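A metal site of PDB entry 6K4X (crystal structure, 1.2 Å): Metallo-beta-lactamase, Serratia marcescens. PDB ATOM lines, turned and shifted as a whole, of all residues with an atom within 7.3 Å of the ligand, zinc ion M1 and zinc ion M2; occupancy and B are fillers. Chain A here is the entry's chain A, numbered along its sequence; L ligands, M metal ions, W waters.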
ATOM      1  N   TRP A   5      -6.826  -8.676  -3.314  1.00  0.00           N
ATOM      2  CA  TRP A   5      -7.556  -9.187  -4.464  1.00  0.00           C
ATOM      3  C   TRP A   5      -8.232 -10.506  -4.177  1.00  0.00           C
ATOM      4  O   TRP A   5      -9.144 -10.878  -4.857  1.00  0.00           O
ATOM      5  CB  TRP A   5      -6.626  -9.438  -5.654  1.00  0.00           C
ATOM      6  CG  TRP A   5      -6.031  -8.235  -6.293  1.00  0.00           C
ATOM      7  CD1 TRP A   5      -6.379  -6.937  -6.103  1.00  0.00           C
ATOM      8  CD2 TRP A   5      -4.935  -8.255  -7.212  1.00  0.00           C
ATOM      9  NE1 TRP A   5      -5.589  -6.137  -6.895  1.00  0.00           N
ATOM     10  CE2 TRP A   5      -4.683  -6.916  -7.560  1.00  0.00           C
ATOM     11  CE3 TRP A   5      -4.138  -9.272  -7.757  1.00  0.00           C
ATOM     12  CZ2 TRP A   5      -3.673  -6.572  -8.459  1.00  0.00           C
ATOM     13  CZ3 TRP A   5      -3.142  -8.929  -8.641  1.00  0.00           C
ATOM     14  CH2 TRP A   5      -2.907  -7.599  -8.977  1.00  0.00           C
ATOM     15  N   ILE A  26     -11.539  -7.186  -5.681  1.00  0.00           N
ATOM     16  CA  ILE A  26     -11.870  -7.379  -7.109  1.00  0.00           C
ATOM     17  C   ILE A  26     -13.351  -7.667  -7.220  1.00  0.00           C
ATOM     18  O   ILE A  26     -13.870  -8.543  -6.515  1.00  0.00           O
ATOM     19  CB  ILE A  26     -11.059  -8.508  -7.765  1.00  0.00           C
ATOM     20  CG1 ILE A  26      -9.548  -8.258  -7.709  1.00  0.00           C
ATOM     21  CG2 ILE A  26     -11.525  -8.713  -9.190  1.00  0.00           C
ATOM     22  CD1 ILE A  26      -9.067  -7.144  -8.595  1.00  0.00           C
ATOM     23  N   HIS A  72     -11.707  -8.752 -18.678  1.00  0.00           N
ATOM     24  CA  HIS A  72     -10.472  -8.943 -19.379  1.00  0.00           C
ATOM     25  C   HIS A  72      -9.604  -9.977 -18.689  1.00  0.00           C
ATOM     26  O   HIS A  72      -9.787 -10.342 -17.528  1.00  0.00           O
ATOM     27  CB  HIS A  72      -9.714  -7.616 -19.608  1.00  0.00           C
ATOM     28  CG  HIS A  72      -9.047  -7.053 -18.404  1.00  0.00           C
ATOM     29  ND1 HIS A  72      -9.649  -6.153 -17.578  1.00  0.00           N
ATOM     30  CD2 HIS A  72      -7.800  -7.246 -17.894  1.00  0.00           C
ATOM     31  CE1 HIS A  72      -8.806  -5.797 -16.627  1.00  0.00           C
ATOM     32  NE2 HIS A  72      -7.634  -6.476 -16.770  1.00  0.00           N
ATOM     33  N   SER A  73      -8.603 -10.446 -19.457  1.00  0.00           N
ATOM     34  CA  SER A  73      -7.845 -11.660 -19.185  1.00  0.00           C
ATOM     35  C   SER A  73      -6.519 -11.359 -18.482  1.00  0.00           C
ATOM     36  O   SER A  73      -5.456 -11.714 -19.007  1.00  0.00           O
ATOM     37  CB  SER A  73      -7.651 -12.377 -20.487  1.00  0.00           C
ATOM     38  OG  SER A  73      -7.166 -11.494 -21.498  1.00  0.00           O
ATOM     39  N   HIS A  74      -6.605 -10.751 -17.290  1.00  0.00           N
ATOM     40  CA  HIS A  74      -5.471 -10.678 -16.377  1.00  0.00           C
ATOM     41  C   HIS A  74      -5.830 -11.447 -15.108  1.00  0.00           C
ATOM     42  O   HIS A  74      -7.001 -11.669 -14.805  1.00  0.00           O
ATOM     43  CB  HIS A  74      -5.100  -9.244 -16.012  1.00  0.00           C
ATOM     44  CG  HIS A  74      -4.584  -8.469 -17.186  1.00  0.00           C
ATOM     45  ND1 HIS A  74      -4.669  -7.120 -17.282  1.00  0.00           N
ATOM     46  CD2 HIS A  74      -3.922  -8.904 -18.271  1.00  0.00           C
ATOM     47  CE1 HIS A  74      -4.099  -6.758 -18.412  1.00  0.00           C
ATOM     48  NE2 HIS A  74      -3.634  -7.826 -19.034  1.00  0.00           N
ATOM     49  N   GLU A  75      -4.795 -11.881 -14.395  1.00  0.00           N
ATOM     50  CA  GLU A  75      -4.931 -12.815 -13.283  1.00  0.00           C
ATOM     51  C   GLU A  75      -5.858 -12.299 -12.186  1.00  0.00           C
ATOM     52  O   GLU A  75      -6.440 -13.105 -11.466  1.00  0.00           O
ATOM     53  CB  GLU A  75      -3.553 -13.151 -12.720  1.00  0.00           C
ATOM     54  CG  GLU A  75      -2.898 -12.012 -11.951  1.00  0.00           C
ATOM     55  CD  GLU A  75      -1.563 -12.260 -11.248  1.00  0.00           C
ATOM     56  OE1 GLU A  75      -1.406 -13.350 -10.683  1.00  0.00           O
ATOM     57  OE2 GLU A  75      -0.695 -11.347 -11.242  1.00  0.00           O
ATOM     58  N   ASP A  76      -5.938 -10.991 -11.976  1.00  0.00           N
ATOM     59  CA  ASP A  76      -6.755 -10.458 -10.901  1.00  0.00           C
ATOM     60  C   ASP A  76      -8.265 -10.590 -11.176  1.00  0.00           C
ATOM     61  O   ASP A  76      -9.033 -10.691 -10.217  1.00  0.00           O
ATOM     62  CB  ASP A  76      -6.382  -9.025 -10.560  1.00  0.00           C
ATOM     63  CG  ASP A  76      -6.399  -8.006 -11.680  1.00  0.00           C
ATOM     64  OD1 ASP A  76      -6.164  -8.394 -12.854  1.00  0.00           O
ATOM     65  OD2 ASP A  76      -6.607  -6.817 -11.361  1.00  0.00           O
ATOM     66  N   HIS A  77      -8.682 -10.519 -12.442  1.00  0.00           N
ATOM     67  CA  HIS A  77     -10.111 -10.614 -12.777  1.00  0.00           C
ATOM     68  C   HIS A  77     -10.486 -12.023 -13.224  1.00  0.00           C
ATOM     69  O   HIS A  77     -11.650 -12.443 -13.069  1.00  0.00           O
ATOM     70  CB  HIS A  77     -10.469  -9.613 -13.875  1.00  0.00           C
ATOM     71  CG  HIS A  77     -10.012  -8.244 -13.531  1.00  0.00           C
ATOM     72  ND1 HIS A  77     -10.674  -7.439 -12.615  1.00  0.00           N
ATOM     73  CD2 HIS A  77      -8.896  -7.582 -13.889  1.00  0.00           C
ATOM     74  CE1 HIS A  77      -9.959  -6.328 -12.468  1.00  0.00           C
ATOM     75  NE2 HIS A  77      -8.858  -6.397 -13.200  1.00  0.00           N
ATOM     76  N   ASP A 111      -0.192  -7.221 -25.444  1.00  0.00           N
ATOM     77  CA  ASP A 111      -0.643  -6.588 -24.195  1.00  0.00           C
ATOM     78  C   ASP A 111       0.431  -5.597 -23.746  1.00  0.00           C
ATOM     79  O   ASP A 111       1.591  -5.979 -23.634  1.00  0.00           O
ATOM     80  CB  ASP A 111      -0.891  -7.668 -23.147  1.00  0.00           C
ATOM     81  CG  ASP A 111      -1.585  -7.175 -21.890  1.00  0.00           C
ATOM     82  OD1 ASP A 111      -1.127  -6.189 -21.296  1.00  0.00           O
ATOM     83  OD2 ASP A 111      -2.590  -7.808 -21.526  1.00  0.00           O
ATOM     84  N   GLN A 113       1.269  -4.687 -20.915  1.00  0.00           N
ATOM     85  CA  GLN A 113       1.956  -5.210 -19.739  1.00  0.00           C
ATOM     86  C   GLN A 113       2.782  -6.459 -20.031  1.00  0.00           C
ATOM     87  O   GLN A 113       3.426  -6.979 -19.116  1.00  0.00           O
ATOM     88  CB  GLN A 113       0.949  -5.483 -18.624  1.00  0.00           C
ATOM     89  CG  GLN A 113       0.360  -4.226 -18.035  1.00  0.00           C
ATOM     90  CD  GLN A 113      -0.577  -4.563 -16.902  1.00  0.00           C
ATOM     91  OE1 GLN A 113      -0.144  -4.829 -15.776  1.00  0.00           O
ATOM     92  NE2 GLN A 113      -1.866  -4.645 -17.170  1.00  0.00           N
ATOM     93  N   SER A 116       5.550  -8.387 -17.809  1.00  0.00           N
ATOM     94  CA  SER A 116       5.364  -8.077 -16.400  1.00  0.00           C
ATOM     95  C   SER A 116       4.126  -8.787 -15.831  1.00  0.00           C
ATOM     96  O   SER A 116       3.812  -8.623 -14.656  1.00  0.00           O
ATOM     97  CB  SER A 116       5.304  -6.588 -16.165  1.00  0.00           C
ATOM     98  OG  SER A 116       4.073  -6.047 -16.647  1.00  0.00           O
ATOM     99  N   LEU A 117       3.431  -9.597 -16.634  1.00  0.00           N
ATOM    100  CA  LEU A 117       2.182 -10.222 -16.190  1.00  0.00           C
ATOM    101  C   LEU A 117       2.464 -11.613 -15.610  1.00  0.00           C
ATOM    102  O   LEU A 117       3.370 -12.302 -16.073  1.00  0.00           O
ATOM    103  CB  LEU A 117       1.197 -10.340 -17.346  1.00  0.00           C
ATOM    104  CG  LEU A 117       0.659  -9.021 -17.872  1.00  0.00           C
ATOM    105  CD1 LEU A 117       0.070  -9.180 -19.270  1.00  0.00           C
ATOM    106  CD2 LEU A 117      -0.365  -8.438 -16.908  1.00  0.00           C
ATOM    107  N   HIS A 150      -6.831  -1.654 -22.648  1.00  0.00           N
ATOM    108  CA  HIS A 150      -6.112  -2.350 -21.570  1.00  0.00           C
ATOM    109  C   HIS A 150      -5.757  -3.784 -21.997  1.00  0.00           C
ATOM    110  O   HIS A 150      -4.687  -4.286 -21.653  1.00  0.00           O
ATOM    111  CB  HIS A 150      -6.893  -2.233 -20.284  1.00  0.00           C
ATOM    112  CG  HIS A 150      -6.292  -2.865 -19.094  1.00  0.00           C
ATOM    113  ND1 HIS A 150      -5.376  -2.205 -18.319  1.00  0.00           N
ATOM    114  CD2 HIS A 150      -6.514  -4.053 -18.503  1.00  0.00           C
ATOM    115  CE1 HIS A 150      -5.077  -2.978 -17.275  1.00  0.00           C
ATOM    116  NE2 HIS A 150      -5.721  -4.142 -17.376  1.00  0.00           N
ATOM    117  N   THR A 151      -6.679  -4.398 -22.737  1.00  0.00           N
ATOM    118  CA  THR A 151      -6.460  -5.646 -23.445  1.00  0.00           C
ATOM    119  C   THR A 151      -7.244  -5.555 -24.749  1.00  0.00           C
ATOM    120  O   THR A 151      -8.216  -4.794 -24.841  1.00  0.00           O
ATOM    121  CB  THR A 151      -6.932  -6.903 -22.676  1.00  0.00           C
ATOM    122  OG1 THR A 151      -8.367  -6.913 -22.604  1.00  0.00           O
ATOM    123  CG2 THR A 151      -6.289  -7.080 -21.325  1.00  0.00           C
ATOM    124  N   ASP A 174     -15.311  -2.684 -17.513  1.00  0.00           N
ATOM    125  CA  ASP A 174     -13.948  -3.161 -17.668  1.00  0.00           C
ATOM    126  C   ASP A 174     -12.974  -2.025 -17.363  1.00  0.00           C
ATOM    127  O   ASP A 174     -13.317  -0.839 -17.384  1.00  0.00           O
ATOM    128  CB  ASP A 174     -13.709  -3.672 -19.080  1.00  0.00           C
ATOM    129  CG  ASP A 174     -12.427  -4.455 -19.237  1.00  0.00           C
ATOM    130  OD1 ASP A 174     -11.914  -4.922 -18.222  1.00  0.00           O
ATOM    131  OD2 ASP A 174     -12.020  -4.637 -20.412  1.00  0.00           O
ATOM    132  N   SER A 175     -11.736  -2.417 -17.040  1.00  0.00           N
ATOM    133  CA  SER A 175     -10.615  -1.480 -16.869  1.00  0.00           C
ATOM    134  C   SER A 175     -10.293  -0.773 -18.173  1.00  0.00           C
ATOM    135  O   SER A 175     -10.178  -1.387 -19.221  1.00  0.00           O
ATOM    136  CB  SER A 175      -9.421  -2.212 -16.347  1.00  0.00           C
ATOM    137  OG  SER A 175      -9.762  -2.868 -15.137  1.00  0.00           O
ATOM    138  N   LEU A 176     -10.071   0.544 -18.059  1.00  0.00           N
ATOM    139  CA  LEU A 176      -9.724   1.400 -19.189  1.00  0.00           C
ATOM    140  C   LEU A 176      -8.340   2.020 -19.003  1.00  0.00           C
ATOM    141  O   LEU A 176      -8.078   3.117 -19.510  1.00  0.00           O
ATOM    142  CB  LEU A 176     -10.772   2.497 -19.319  1.00  0.00           C
ATOM    143  CG  LEU A 176     -12.210   2.039 -19.466  1.00  0.00           C
ATOM    144  CD1 LEU A 176     -13.132   3.241 -19.589  1.00  0.00           C
ATOM    145  CD2 LEU A 176     -12.380   1.080 -20.643  1.00  0.00           C
ATOM    146  N   THR A 177      -7.462   1.327 -18.263  1.00  0.00           N
ATOM    147  CA  THR A 177      -6.229   1.918 -17.772  1.00  0.00           C
ATOM    148  C   THR A 177      -5.052   1.622 -18.712  1.00  0.00           C
ATOM    149  O   THR A 177      -4.745   0.485 -19.063  1.00  0.00           O
ATOM    150  CB  THR A 177      -5.933   1.362 -16.380  1.00  0.00           C
ATOM    151  OG1 THR A 177      -5.972  -0.055 -16.459  1.00  0.00           O
ATOM    152  CG2 THR A 177      -6.919   1.879 -15.359  1.00  0.00           C
ATOM    153  N   ALA A 178      -4.310   2.682 -19.020  1.00  0.00           N
ATOM    154  CA  ALA A 178      -3.041   2.626 -19.739  1.00  0.00           C
ATOM    155  C   ALA A 178      -1.938   2.336 -18.723  1.00  0.00           C
ATOM    156  O   ALA A 178      -1.564   3.192 -17.877  1.00  0.00           O
ATOM    157  CB  ALA A 178      -2.786   3.935 -20.454  1.00  0.00           C
ATOM    158  N   VAL A 179      -1.471   1.099 -18.716  1.00  0.00           N
ATOM    159  CA  VAL A 179      -0.393   0.631 -17.809  1.00  0.00           C
ATOM    160  C   VAL A 179       0.463  -0.328 -18.630  1.00  0.00           C
ATOM    161  O   VAL A 179      -0.018  -0.979 -19.532  1.00  0.00           O
ATOM    162  CB  VAL A 179      -0.998  -0.033 -16.548  1.00  0.00           C
ATOM    163  CG1 VAL A 179      -1.991  -1.108 -16.919  1.00  0.00           C
ATOM    164  CG2 VAL A 179       0.015  -0.620 -15.570  1.00  0.00           C
ATOM    165  N   SER A 180       1.759  -0.373 -18.348  1.00  0.00           N
ATOM    166  CA  SER A 180       2.613  -1.191 -19.192  1.00  0.00           C
ATOM    167  C   SER A 180       3.839  -1.679 -18.448  1.00  0.00           C
ATOM    168  O   SER A 180       4.168  -1.202 -17.367  1.00  0.00           O
ATOM    169  CB  SER A 180       3.050  -0.422 -20.407  1.00  0.00           C
ATOM    170  OG  SER A 180       4.065   0.529 -20.075  1.00  0.00           O
ATOM    171  N   ALA A 214     -14.494  -3.080 -12.407  1.00  0.00           N
ATOM    172  CA  ALA A 214     -13.792  -4.319 -12.185  1.00  0.00           C
ATOM    173  C   ALA A 214     -12.880  -4.226 -10.947  1.00  0.00           C
ATOM    174  O   ALA A 214     -12.812  -5.158 -10.136  1.00  0.00           O
ATOM    175  CB  ALA A 214     -13.031  -4.703 -13.433  1.00  0.00           C
ATOM    176  N   HIS A 215     -12.158  -3.115 -10.808  1.00  0.00           N
ATOM    177  CA  HIS A 215     -11.571  -2.711  -9.535  1.00  0.00           C
ATOM    178  C   HIS A 215     -12.589  -1.851  -8.804  1.00  0.00           C
ATOM    179  O   HIS A 215     -12.871  -0.731  -9.224  1.00  0.00           O
ATOM    180  CB  HIS A 215     -10.259  -1.949  -9.733  1.00  0.00           C
ATOM    181  CG  HIS A 215      -9.146  -2.844 -10.186  1.00  0.00           C
ATOM    182  ND1 HIS A 215      -8.399  -3.601  -9.298  1.00  0.00           N
ATOM    183  CD2 HIS A 215      -8.714  -3.188 -11.425  1.00  0.00           C
ATOM    184  CE1 HIS A 215      -7.555  -4.357  -9.976  1.00  0.00           C
ATOM    185  NE2 HIS A 215      -7.716  -4.126 -11.280  1.00  0.00           N
ATOM    186  N   VAL A 218     -12.690   1.986  -8.151  1.00  0.00           N
ATOM    187  CA  VAL A 218     -12.722   2.914  -9.235  1.00  0.00           C
ATOM    188  C   VAL A 218     -14.015   3.745  -9.203  1.00  0.00           C
ATOM    189  O   VAL A 218     -13.985   4.926  -9.551  1.00  0.00           O
ATOM    190  CB  VAL A 218     -12.523   2.187 -10.572  1.00  0.00           C
ATOM    191  CG1 VAL A 218     -12.956   3.017 -11.768  1.00  0.00           C
ATOM    192  CG2 VAL A 218     -11.073   1.771 -10.715  1.00  0.00           C
ATOM    193  N   ARG A 252      -5.521   9.267 -17.412  1.00  0.00           N
ATOM    194  CA  ARG A 252      -4.368   8.409 -17.208  1.00  0.00           C
ATOM    195  C   ARG A 252      -3.589   8.259 -18.524  1.00  0.00           C
ATOM    196  O   ARG A 252      -2.351   8.300 -18.513  1.00  0.00           O
ATOM    197  CB  ARG A 252      -4.820   7.046 -16.678  1.00  0.00           C
ATOM    198  CG  ARG A 252      -3.696   6.098 -16.344  1.00  0.00           C
ATOM    199  CD  ARG A 252      -4.209   4.881 -15.595  1.00  0.00           C
ATOM    200  NE  ARG A 252      -3.112   4.013 -15.203  1.00  0.00           N
ATOM    201  CZ  ARG A 252      -3.118   3.163 -14.201  1.00  0.00           C
ATOM    202  NH1 ARG A 252      -4.185   3.046 -13.434  1.00  0.00           N
ATOM    203  NH2 ARG A 252      -2.068   2.385 -14.016  1.00  0.00           N
HETATM  204  O1  LIG L   1      -7.381  -3.640 -14.177  1.00  0.00           O
HETATM  205  C1  LIG L   1      -6.608  -2.653 -14.131  1.00  0.00           C
HETATM  206  O2  LIG L   1      -7.022  -1.474 -14.333  1.00  0.00           O
HETATM  207  C2  LIG L   1      -5.161  -2.824 -13.858  1.00  0.00           C
HETATM  208  C3  LIG L   1      -4.434  -1.622 -13.579  1.00  0.00           C
HETATM  209  C4  LIG L   1      -4.501  -4.059 -13.843  1.00  0.00           C
HETATM  210  S1  LIG L   1      -5.155  -5.628 -14.035  1.00  0.00           S
HETATM  211  C5  LIG L   1      -3.105  -4.053 -13.592  1.00  0.00           C
HETATM  212  C6  LIG L   1      -2.390  -2.871 -13.337  1.00  0.00           C
HETATM  213  N1  LIG L   1      -1.030  -2.911 -13.053  1.00  0.00           N
HETATM  214  C7  LIG L   1      -3.069  -1.684 -13.304  1.00  0.00           C
HETATM  215 ZN    ZN M   1      -5.820  -5.780 -16.210  1.00  0.00          ZN
HETATM  216 ZN    ZN M   2      -7.133  -5.400 -12.771  1.00  0.00          ZN
HETATM  217  O   HOH W   1       0.790  -0.561 -12.433  1.00  0.00           O
HETATM  218  O   HOH W   2      -9.147   0.129 -13.455  1.00  0.00           O
HETATM  219  O   HOH W   3      -4.413  -4.819 -10.764  1.00  0.00           O
HETATM  220  O   HOH W   4      -5.419  -1.733 -10.340  1.00  0.00           O
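An oxygen (O2) of the ligand sits at hydrogen-bond distance from the side-chain hydroxyl (OG) of Ser 175 (3.2 Å).
OG1 of Thr 177 is in hydrogen-bond range of O2 of the ligand.
A nitrogen (N1) of the ligand lies within hydrogen-bond range of the side-chain amide oxygen (OE1) of Gln 113.
A ring nitrogen (ND1) of His 150 lies within hydrogen-bond range of the backbone carbonyl oxygen (O) of Thr 177 (2.9 Å).
A ring nitrogen (ND1) of His 72 lies within hydrogen-bond range of the side-chain carboxylate of Asp 174 (2.7 Å).
NE2 of His 74 lies within hydrogen-bond range of OD2 of Asp 111, 2.7 Å away.
OD1 of Asp 111 is in hydrogen-bond range of N of Gln 113, at 2.9 Å.
OG of Ser 116 sits at hydrogen-bond distance from O of Gln 113, at 2.7 Å.
Val 179 touches the ligand.
The nearest printed residue that does not touch the ligand is Arg 252 (4.3 Å).
Of the 25 residues printed, 3 come within 4 Å of zinc ion M2.
NE2 of His 150 binds zinc ion M1 (2.0 Å).
Zinc ion M1 is bound by NE2 of His 72 (2.0 Å).
Zinc ion M1 is bound by a ring nitrogen (ND1) of His 74.
Zinc ion M1 is bound by S1 of the ligand (2.3 Å).
Zinc ion M2 is bound by NE2 of His 77, NE2 of His 215, OD2 of Asp 76, O1 of the ligand and S1 of the ligand.
Zinc ion M2 has five donor atoms within binding distance.
Water W2 bridges O2 of the ligand (2.8 Å) and OG of Ser 175 (3.5 Å).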
